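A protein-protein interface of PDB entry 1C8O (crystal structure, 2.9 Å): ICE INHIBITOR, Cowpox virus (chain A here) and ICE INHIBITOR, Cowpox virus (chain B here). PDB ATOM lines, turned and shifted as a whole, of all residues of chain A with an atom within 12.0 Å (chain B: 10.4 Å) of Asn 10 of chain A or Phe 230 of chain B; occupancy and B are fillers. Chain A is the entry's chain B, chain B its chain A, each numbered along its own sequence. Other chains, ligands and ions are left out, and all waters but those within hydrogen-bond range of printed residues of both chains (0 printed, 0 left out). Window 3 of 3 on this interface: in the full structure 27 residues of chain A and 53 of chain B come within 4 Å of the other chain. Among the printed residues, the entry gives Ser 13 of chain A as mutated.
The backbone NH (N) of Asp 232 of chain B sits at hydrogen-bond distance from the backbone carbonyl oxygen (O) of Asn 10 of chain A, 3.1 Å away.
O of Asp 232 of chain B lies within hydrogen-bond range of N of Phe 12 of chain A (3.0 Å).
O of Phe 12 of chain A is in hydrogen-bond range of N of His 234 of chain B (3.0 Å).
The backbone carbonyl oxygen (O) of His 234 of chain B sits at hydrogen-bond distance from the backbone NH (N) of Ala 14 of chain A, 2.7 Å away.
The backbone NH of Val 233 of chain B is in hydrogen-bond range of the backbone carbonyl oxygen of Met 166 of chain B (2.9 Å).
OH of Tyr 167 of chain B is in hydrogen-bond range of NE2 of His 234 of chain B, 2.9 Å away.
The backbone NH of Leu 200 of chain B is in hydrogen-bond range of the backbone carbonyl oxygen of Ser 184 of chain B (2.9 Å).
OG of Ser 184 of chain B sits at hydrogen-bond distance from OD1 of Asp 202 of chain B.
The side-chain carboxylate of Glu 11 of chain A lies close to the side-chain hydroxyl of Ser 13 of chain A (3.4 Å).
Among the printed residues, merely in contact across the chains: Ser 13 of chain A with Leu 200 of chain B (2.9 Å), Phe 12 of chain A with Leu 200 of chain B (3.2 Å), Asn 10 of chain A with Ile 231 of chain B (3.3 Å), Glu 11 of chain A with Ile 231 of chain B (3.6 Å), Asn 10 of chain A with Phe 230 of chain B (3.6 Å), Glu 11 of chain A with Asp 232 of chain B (3.6 Å), Ser 13 of chain A with His 234 of chain B (3.6 Å), Phe 12 of chain A with Ile 186 of chain B (3.6 Å), Phe 12 of chain A with Val 233 of chain B (3.7 Å), Ala 14 of chain A with Leu 200 of chain B (3.8 Å), Glu 11 of chain A with His 234 of chain B (3.9 Å) and Phe 12 of chain A with Ser 184 of chain B (3.9 Å).
Of the printed residues of chain B, Glu 11 of chain A touches Ile 231, Asp 232 and His 234.
Of the printed residues of chain B, Phe 12 of chain A touches Ser 184 (3.9 Å), Ile 186 (3.6 Å), Leu 200 (3.2 Å), Asp 232 (3.0 Å), Val 233 (3.7 Å) and His 234 (3.0 Å).
No residue of chain A comes within 4 Å of Gly 168 of chain B.
Asn 172 of chain B touches none of the printed residues of chain A.
Ile 185 of chain B touches none of the printed residues of chain A.
No residue of chain A comes within 4 Å of Ala 228 of chain B.
No residue of chain A comes within 4 Å of Met 229 of chain B.
The nearest residue of chain B that does not touch Asn 10 of chain A is Val 233 of chain B (6.2 Å).
Of the 5 printed residues of chain A, 5 touch a printed residue of chain B.
Printed residues of chain B that touch a printed residue of chain A: Ser 184, Ile 186, Leu 200, Phe 230, Ile 231, Asp 232, Val 233 and His 234.
Among the printed residues, no Asp or Glu carboxylate lies within 4 Å of a Lys or Arg side-chain nitrogen of the other chain.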
ATOM      1  N   ASN A  10     -24.767 -28.485  11.572  1.00  0.00           N
ATOM      2  CA  ASN A  10     -25.984 -28.264  12.416  1.00  0.00           C
ATOM      3  C   ASN A  10     -26.087 -29.265  13.587  1.00  0.00           C
ATOM      4  O   ASN A  10     -27.104 -29.944  13.776  1.00  0.00           O
ATOM      5  CB  ASN A  10     -27.253 -28.284  11.528  1.00  0.00           C
ATOM      6  CG  ASN A  10     -27.406 -29.570  10.712  1.00  0.00           C
ATOM      7  OD1 ASN A  10     -26.443 -30.316  10.501  1.00  0.00           O
ATOM      8  ND2 ASN A  10     -28.629 -29.819  10.233  1.00  0.00           N
ATOM      9  N   GLU A  11     -25.014 -29.321  14.376  1.00  0.00           N
ATOM     10  CA  GLU A  11     -24.906 -30.201  15.540  1.00  0.00           C
ATOM     11  C   GLU A  11     -24.137 -29.553  16.701  1.00  0.00           C
ATOM     12  O   GLU A  11     -22.973 -29.193  16.559  1.00  0.00           O
ATOM     13  CB  GLU A  11     -24.219 -31.509  15.144  1.00  0.00           C
ATOM     14  CG  GLU A  11     -23.854 -32.411  16.310  1.00  0.00           C
ATOM     15  CD  GLU A  11     -23.454 -33.808  15.873  1.00  0.00           C
ATOM     16  OE1 GLU A  11     -24.354 -34.651  15.611  1.00  0.00           O
ATOM     17  OE2 GLU A  11     -22.228 -34.058  15.783  1.00  0.00           O
ATOM     18  N   PHE A  12     -24.803 -29.419  17.846  1.00  0.00           N
ATOM     19  CA  PHE A  12     -24.215 -28.832  19.050  1.00  0.00           C
ATOM     20  C   PHE A  12     -23.831 -29.975  19.999  1.00  0.00           C
ATOM     21  O   PHE A  12     -24.687 -30.495  20.719  1.00  0.00           O
ATOM     22  CB  PHE A  12     -25.251 -27.907  19.701  1.00  0.00           C
ATOM     23  CG  PHE A  12     -24.737 -27.126  20.886  1.00  0.00           C
ATOM     24  CD1 PHE A  12     -24.543 -27.739  22.120  1.00  0.00           C
ATOM     25  CD2 PHE A  12     -24.469 -25.766  20.772  1.00  0.00           C
ATOM     26  CE1 PHE A  12     -24.092 -27.010  23.217  1.00  0.00           C
ATOM     27  CE2 PHE A  12     -24.019 -25.032  21.864  1.00  0.00           C
ATOM     28  CZ  PHE A  12     -23.830 -25.655  23.087  1.00  0.00           C
ATOM     29  N   SER A  13     -22.554 -30.370  19.986  1.00  0.00           N
ATOM     30  CA  SER A  13     -22.053 -31.460  20.842  1.00  0.00           C
ATOM     31  C   SER A  13     -21.211 -30.937  22.001  1.00  0.00           C
ATOM     32  O   SER A  13     -20.076 -30.498  21.799  1.00  0.00           O
ATOM     33  CB  SER A  13     -21.197 -32.440  20.032  1.00  0.00           C
ATOM     34  OG  SER A  13     -21.938 -33.023  18.977  1.00  0.00           O
ATOM     35  N   ALA A  14     -21.756 -31.006  23.212  1.00  0.00           N
ATOM     36  CA  ALA A  14     -21.056 -30.507  24.390  1.00  0.00           C
ATOM     37  C   ALA A  14     -20.106 -31.531  24.995  1.00  0.00           C
ATOM     38  O   ALA A  14     -20.224 -31.872  26.167  1.00  0.00           O
ATOM     39  CB  ALA A  14     -22.067 -30.039  25.436  1.00  0.00           C
ATOM     40  N   MET B 166     -30.800 -35.336  21.597  1.00  0.00           N
ATOM     41  CA  MET B 166     -32.113 -35.186  21.005  1.00  0.00           C
ATOM     42  C   MET B 166     -32.023 -34.599  19.607  1.00  0.00           C
ATOM     43  O   MET B 166     -31.298 -33.629  19.362  1.00  0.00           O
ATOM     44  CB  MET B 166     -33.019 -34.346  21.890  1.00  0.00           C
ATOM     45  CG  MET B 166     -32.797 -32.872  21.825  1.00  0.00           C
ATOM     46  SD  MET B 166     -34.218 -32.142  22.615  1.00  0.00           S
ATOM     47  CE  MET B 166     -35.531 -32.835  21.597  1.00  0.00           C
ATOM     48  N   TYR B 167     -32.771 -35.214  18.696  1.00  0.00           N
ATOM     49  CA  TYR B 167     -32.776 -34.820  17.302  1.00  0.00           C
ATOM     50  C   TYR B 167     -34.148 -34.417  16.764  1.00  0.00           C
ATOM     51  O   TYR B 167     -35.187 -34.718  17.365  1.00  0.00           O
ATOM     52  CB  TYR B 167     -32.225 -35.963  16.454  1.00  0.00           C
ATOM     53  CG  TYR B 167     -31.000 -36.651  17.034  1.00  0.00           C
ATOM     54  CD1 TYR B 167     -31.121 -37.738  17.904  1.00  0.00           C
ATOM     55  CD2 TYR B 167     -29.718 -36.248  16.669  1.00  0.00           C
ATOM     56  CE1 TYR B 167     -29.986 -38.407  18.384  1.00  0.00           C
ATOM     57  CE2 TYR B 167     -28.583 -36.908  17.141  1.00  0.00           C
ATOM     58  CZ  TYR B 167     -28.722 -37.984  17.989  1.00  0.00           C
ATOM     59  OH  TYR B 167     -27.587 -38.641  18.403  1.00  0.00           O
ATOM     60  N   GLY B 168     -34.124 -33.729  15.621  1.00  0.00           N
ATOM     61  CA  GLY B 168     -35.340 -33.279  14.960  1.00  0.00           C
ATOM     62  C   GLY B 168     -36.008 -32.061  15.569  1.00  0.00           C
ATOM     63  O   GLY B 168     -37.102 -31.686  15.158  1.00  0.00           O
ATOM     64  N   GLU B 169     -35.361 -31.432  16.538  1.00  0.00           N
ATOM     65  CA  GLU B 169     -35.945 -30.269  17.188  1.00  0.00           C
ATOM     66  C   GLU B 169     -35.282 -28.950  16.813  1.00  0.00           C
ATOM     67  O   GLU B 169     -34.147 -28.911  16.319  1.00  0.00           O
ATOM     68  CB  GLU B 169     -35.886 -30.442  18.704  1.00  0.00           C
ATOM     69  CG  GLU B 169     -37.201 -30.791  19.346  1.00  0.00           C
ATOM     70  CD  GLU B 169     -37.782 -32.093  18.838  1.00  0.00           C
ATOM     71  OE1 GLU B 169     -37.066 -33.123  18.837  1.00  0.00           O
ATOM     72  OE2 GLU B 169     -38.968 -32.094  18.448  1.00  0.00           O
ATOM     73  N   ALA B 170     -36.001 -27.864  17.057  1.00  0.00           N
ATOM     74  CA  ALA B 170     -35.474 -26.548  16.766  1.00  0.00           C
ATOM     75  C   ALA B 170     -35.227 -25.833  18.081  1.00  0.00           C
ATOM     76  O   ALA B 170     -36.012 -25.948  19.016  1.00  0.00           O
ATOM     77  CB  ALA B 170     -36.456 -25.769  15.910  1.00  0.00           C
ATOM     78  N   PHE B 171     -34.122 -25.107  18.152  1.00  0.00           N
ATOM     79  CA  PHE B 171     -33.766 -24.375  19.353  1.00  0.00           C
ATOM     80  C   PHE B 171     -33.180 -23.056  18.917  1.00  0.00           C
ATOM     81  O   PHE B 171     -32.747 -22.921  17.783  1.00  0.00           O
ATOM     82  CB  PHE B 171     -32.691 -25.121  20.149  1.00  0.00           C
ATOM     83  CG  PHE B 171     -33.142 -26.419  20.720  1.00  0.00           C
ATOM     84  CD1 PHE B 171     -34.081 -26.451  21.739  1.00  0.00           C
ATOM     85  CD2 PHE B 171     -32.616 -27.619  20.253  1.00  0.00           C
ATOM     86  CE1 PHE B 171     -34.493 -27.670  22.289  1.00  0.00           C
ATOM     87  CE2 PHE B 171     -33.019 -28.840  20.792  1.00  0.00           C
ATOM     88  CZ  PHE B 171     -33.957 -28.867  21.808  1.00  0.00           C
ATOM     89  N   ASN B 172     -33.147 -22.094  19.828  1.00  0.00           N
ATOM     90  CA  ASN B 172     -32.567 -20.802  19.523  1.00  0.00           C
ATOM     91  C   ASN B 172     -31.057 -20.921  19.564  1.00  0.00           C
ATOM     92  O   ASN B 172     -30.442 -20.927  20.628  1.00  0.00           O
ATOM     93  CB  ASN B 172     -33.044 -19.751  20.513  1.00  0.00           C
ATOM     94  CG  ASN B 172     -34.365 -19.138  20.101  1.00  0.00           C
ATOM     95  OD1 ASN B 172     -35.350 -19.843  19.851  1.00  0.00           O
ATOM     96  ND2 ASN B 172     -34.391 -17.812  20.016  1.00  0.00           N
ATOM     97  N   HIS B 173     -30.471 -21.018  18.382  1.00  0.00           N
ATOM     98  CA  HIS B 173     -29.040 -21.171  18.226  1.00  0.00           C
ATOM     99  C   HIS B 173     -28.406 -19.864  17.766  1.00  0.00           C
ATOM    100  O   HIS B 173     -29.090 -18.864  17.614  1.00  0.00           O
ATOM    101  CB  HIS B 173     -28.793 -22.295  17.219  1.00  0.00           C
ATOM    102  CG  HIS B 173     -27.353 -22.613  16.995  1.00  0.00           C
ATOM    103  ND1 HIS B 173     -26.537 -21.835  16.203  1.00  0.00           N
ATOM    104  CD2 HIS B 173     -26.581 -23.623  17.458  1.00  0.00           C
ATOM    105  CE1 HIS B 173     -25.322 -22.354  16.186  1.00  0.00           C
ATOM    106  NE2 HIS B 173     -25.321 -23.440  16.939  1.00  0.00           N
ATOM    107  N   ALA B 174     -27.093 -19.886  17.567  1.00  0.00           N
ATOM    108  CA  ALA B 174     -26.322 -18.732  17.126  1.00  0.00           C
ATOM    109  C   ALA B 174     -24.860 -19.137  17.080  1.00  0.00           C
ATOM    110  O   ALA B 174     -24.388 -19.878  17.943  1.00  0.00           O
ATOM    111  CB  ALA B 174     -26.501 -17.595  18.077  1.00  0.00           C
ATOM    112  N   SER B 175     -24.142 -18.661  16.071  1.00  0.00           N
ATOM    113  CA  SER B 175     -22.738 -18.996  15.938  1.00  0.00           C
ATOM    114  C   SER B 175     -21.874 -17.777  16.031  1.00  0.00           C
ATOM    115  O   SER B 175     -21.358 -17.319  15.026  1.00  0.00           O
ATOM    116  CB  SER B 175     -22.454 -19.678  14.604  1.00  0.00           C
ATOM    117  OG  SER B 175     -22.943 -21.003  14.602  1.00  0.00           O
ATOM    118  N   SER B 184     -20.554 -21.485  19.781  1.00  0.00           N
ATOM    119  CA  SER B 184     -21.957 -21.626  19.435  1.00  0.00           C
ATOM    120  C   SER B 184     -22.675 -21.404  20.757  1.00  0.00           C
ATOM    121  O   SER B 184     -22.118 -21.678  21.813  1.00  0.00           O
ATOM    122  CB  SER B 184     -22.239 -23.037  18.925  1.00  0.00           C
ATOM    123  OG  SER B 184     -21.415 -23.341  17.816  1.00  0.00           O
ATOM    124  N   ILE B 185     -23.906 -20.918  20.706  1.00  0.00           N
ATOM    125  CA  ILE B 185     -24.642 -20.655  21.922  1.00  0.00           C
ATOM    126  C   ILE B 185     -26.060 -21.146  21.658  1.00  0.00           C
ATOM    127  O   ILE B 185     -26.637 -20.808  20.646  1.00  0.00           O
ATOM    128  CB  ILE B 185     -24.548 -19.136  22.215  1.00  0.00           C
ATOM    129  CG1 ILE B 185     -24.952 -18.828  23.643  1.00  0.00           C
ATOM    130  CG2 ILE B 185     -25.412 -18.362  21.250  1.00  0.00           C
ATOM    131  CD1 ILE B 185     -26.394 -19.092  23.942  1.00  0.00           C
ATOM    132  N   ILE B 186     -26.618 -21.961  22.544  1.00  0.00           N
ATOM    133  CA  ILE B 186     -27.953 -22.498  22.312  1.00  0.00           C
ATOM    134  C   ILE B 186     -28.826 -22.360  23.557  1.00  0.00           C
ATOM    135  O   ILE B 186     -28.310 -22.163  24.657  1.00  0.00           O
ATOM    136  CB  ILE B 186     -27.833 -23.970  21.910  1.00  0.00           C
ATOM    137  CG1 ILE B 186     -29.130 -24.460  21.278  1.00  0.00           C
ATOM    138  CG2 ILE B 186     -27.422 -24.783  23.110  1.00  0.00           C
ATOM    139  CD1 ILE B 186     -30.023 -25.292  22.159  1.00  0.00           C
ATOM    140  N   LEU B 200     -20.812 -23.148  23.979  1.00  0.00           N
ATOM    141  CA  LEU B 200     -19.839 -24.181  23.619  1.00  0.00           C
ATOM    142  C   LEU B 200     -18.761 -23.721  22.611  1.00  0.00           C
ATOM    143  O   LEU B 200     -19.041 -23.587  21.426  1.00  0.00           O
ATOM    144  CB  LEU B 200     -20.607 -25.366  23.045  1.00  0.00           C
ATOM    145  CG  LEU B 200     -19.742 -26.503  22.559  1.00  0.00           C
ATOM    146  CD1 LEU B 200     -18.889 -26.967  23.707  1.00  0.00           C
ATOM    147  CD2 LEU B 200     -20.606 -27.626  22.020  1.00  0.00           C
ATOM    148  N   ASP B 202     -16.118 -23.452  19.741  1.00  0.00           N
ATOM    149  CA  ASP B 202     -16.025 -24.283  18.550  1.00  0.00           C
ATOM    150  C   ASP B 202     -14.804 -25.177  18.580  1.00  0.00           C
ATOM    151  O   ASP B 202     -14.850 -26.298  18.097  1.00  0.00           O
ATOM    152  CB  ASP B 202     -16.022 -23.426  17.287  1.00  0.00           C
ATOM    153  CG  ASP B 202     -17.375 -22.773  17.013  1.00  0.00           C
ATOM    154  OD1 ASP B 202     -18.414 -23.478  17.080  1.00  0.00           O
ATOM    155  OD2 ASP B 202     -17.401 -21.552  16.715  1.00  0.00           O
ATOM    156  N   MET B 226     -29.524 -14.815  18.940  1.00  0.00           N
ATOM    157  CA  MET B 226     -29.998 -16.177  18.718  1.00  0.00           C
ATOM    158  C   MET B 226     -31.312 -16.233  17.941  1.00  0.00           C
ATOM    159  O   MET B 226     -32.212 -15.428  18.169  1.00  0.00           O
ATOM    160  CB  MET B 226     -30.147 -16.929  20.045  1.00  0.00           C
ATOM    161  CG  MET B 226     -28.861 -17.034  20.859  1.00  0.00           C
ATOM    162  SD  MET B 226     -28.941 -18.368  22.082  1.00  0.00           S
ATOM    163  CE  MET B 226     -30.563 -18.113  22.831  1.00  0.00           C
ATOM    164  N   ASP B 227     -31.402 -17.198  17.022  1.00  0.00           N
ATOM    165  CA  ASP B 227     -32.579 -17.396  16.170  1.00  0.00           C
ATOM    166  C   ASP B 227     -32.984 -18.871  16.168  1.00  0.00           C
ATOM    167  O   ASP B 227     -32.148 -19.737  16.389  1.00  0.00           O
ATOM    168  CB  ASP B 227     -32.258 -16.991  14.723  1.00  0.00           C
ATOM    169  CG  ASP B 227     -31.815 -15.546  14.592  1.00  0.00           C
ATOM    170  OD1 ASP B 227     -32.681 -14.654  14.715  1.00  0.00           O
ATOM    171  OD2 ASP B 227     -30.605 -15.305  14.364  1.00  0.00           O
ATOM    172  N   ALA B 228     -34.263 -19.143  15.896  1.00  0.00           N
ATOM    173  CA  ALA B 228     -34.783 -20.515  15.844  1.00  0.00           C
ATOM    174  C   ALA B 228     -34.088 -21.268  14.721  1.00  0.00           C
ATOM    175  O   ALA B 228     -34.252 -20.952  13.546  1.00  0.00           O
ATOM    176  CB  ALA B 228     -36.282 -20.511  15.616  1.00  0.00           C
ATOM    177  N   MET B 229     -33.322 -22.281  15.095  1.00  0.00           N
ATOM    178  CA  MET B 229     -32.554 -23.057  14.143  1.00  0.00           C
ATOM    179  C   MET B 229     -32.795 -24.536  14.424  1.00  0.00           C
ATOM    180  O   MET B 229     -33.315 -24.894  15.480  1.00  0.00           O
ATOM    181  CB  MET B 229     -31.081 -22.692  14.339  1.00  0.00           C
ATOM    182  CG  MET B 229     -30.129 -23.042  13.211  1.00  0.00           C
ATOM    183  SD  MET B 229     -28.419 -22.436  13.555  1.00  0.00           S
ATOM    184  CE  MET B 229     -28.605 -20.578  13.379  1.00  0.00           C
ATOM    185  N   PHE B 230     -32.445 -25.389  13.471  1.00  0.00           N
ATOM    186  CA  PHE B 230     -32.589 -26.829  13.643  1.00  0.00           C
ATOM    187  C   PHE B 230     -31.193 -27.372  13.956  1.00  0.00           C
ATOM    188  O   PHE B 230     -30.291 -27.296  13.127  1.00  0.00           O
ATOM    189  CB  PHE B 230     -33.107 -27.487  12.362  1.00  0.00           C
ATOM    190  CG  PHE B 230     -34.575 -27.300  12.122  1.00  0.00           C
ATOM    191  CD1 PHE B 230     -35.509 -27.860  12.983  1.00  0.00           C
ATOM    192  CD2 PHE B 230     -35.030 -26.593  11.011  1.00  0.00           C
ATOM    193  CE1 PHE B 230     -36.882 -27.724  12.750  1.00  0.00           C
ATOM    194  CE2 PHE B 230     -36.402 -26.449  10.763  1.00  0.00           C
ATOM    195  CZ  PHE B 230     -37.331 -27.018  11.635  1.00  0.00           C
ATOM    196  N   ILE B 231     -30.992 -27.888  15.160  1.00  0.00           N
ATOM    197  CA  ILE B 231     -29.689 -28.446  15.512  1.00  0.00           C
ATOM    198  C   ILE B 231     -29.937 -29.689  16.312  1.00  0.00           C
ATOM    199  O   ILE B 231     -30.908 -29.769  17.063  1.00  0.00           O
ATOM    200  CB  ILE B 231     -28.802 -27.512  16.397  1.00  0.00           C
ATOM    201  CG1 ILE B 231     -29.571 -26.264  16.800  1.00  0.00           C
ATOM    202  CG2 ILE B 231     -27.518 -27.150  15.656  1.00  0.00           C
ATOM    203  CD1 ILE B 231     -30.781 -26.547  17.629  1.00  0.00           C
ATOM    204  N   ASP B 232     -29.067 -30.668  16.125  1.00  0.00           N
ATOM    205  CA  ASP B 232     -29.170 -31.901  16.862  1.00  0.00           C
ATOM    206  C   ASP B 232     -28.393 -31.615  18.134  1.00  0.00           C
ATOM    207  O   ASP B 232     -27.303 -31.047  18.056  1.00  0.00           O
ATOM    208  CB  ASP B 232     -28.548 -33.037  16.053  1.00  0.00           C
ATOM    209  CG  ASP B 232     -29.524 -33.630  15.043  1.00  0.00           C
ATOM    210  OD1 ASP B 232     -29.128 -34.560  14.298  1.00  0.00           O
ATOM    211  OD2 ASP B 232     -30.692 -33.172  15.007  1.00  0.00           O
ATOM    212  N   VAL B 233     -28.948 -31.963  19.299  1.00  0.00           N
ATOM    213  CA  VAL B 233     -28.241 -31.669  20.547  1.00  0.00           C
ATOM    214  C   VAL B 233     -27.636 -32.851  21.293  1.00  0.00           C
ATOM    215  O   VAL B 233     -28.189 -33.946  21.321  1.00  0.00           O
ATOM    216  CB  VAL B 233     -29.115 -30.861  21.527  1.00  0.00           C
ATOM    217  CG1 VAL B 233     -28.263 -30.384  22.701  1.00  0.00           C
ATOM    218  CG2 VAL B 233     -29.704 -29.662  20.824  1.00  0.00           C
ATOM    219  N   HIS B 234     -26.468 -32.601  21.870  1.00  0.00           N
ATOM    220  CA  HIS B 234     -25.731 -33.592  22.641  1.00  0.00           C
ATOM    221  C   HIS B 234     -25.168 -32.853  23.846  1.00  0.00           C
ATOM    222  O   HIS B 234     -24.155 -32.159  23.741  1.00  0.00           O
ATOM    223  CB  HIS B 234     -24.579 -34.169  21.821  1.00  0.00           C
ATOM    224  CG  HIS B 234     -24.980 -35.268  20.890  1.00  0.00           C
ATOM    225  ND1 HIS B 234     -24.717 -35.229  19.538  1.00  0.00           N
ATOM    226  CD2 HIS B 234     -25.546 -36.474  21.126  1.00  0.00           C
ATOM    227  CE1 HIS B 234     -25.097 -36.365  18.982  1.00  0.00           C
ATOM    228  NE2 HIS B 234     -25.604 -37.139  19.925  1.00  0.00           N
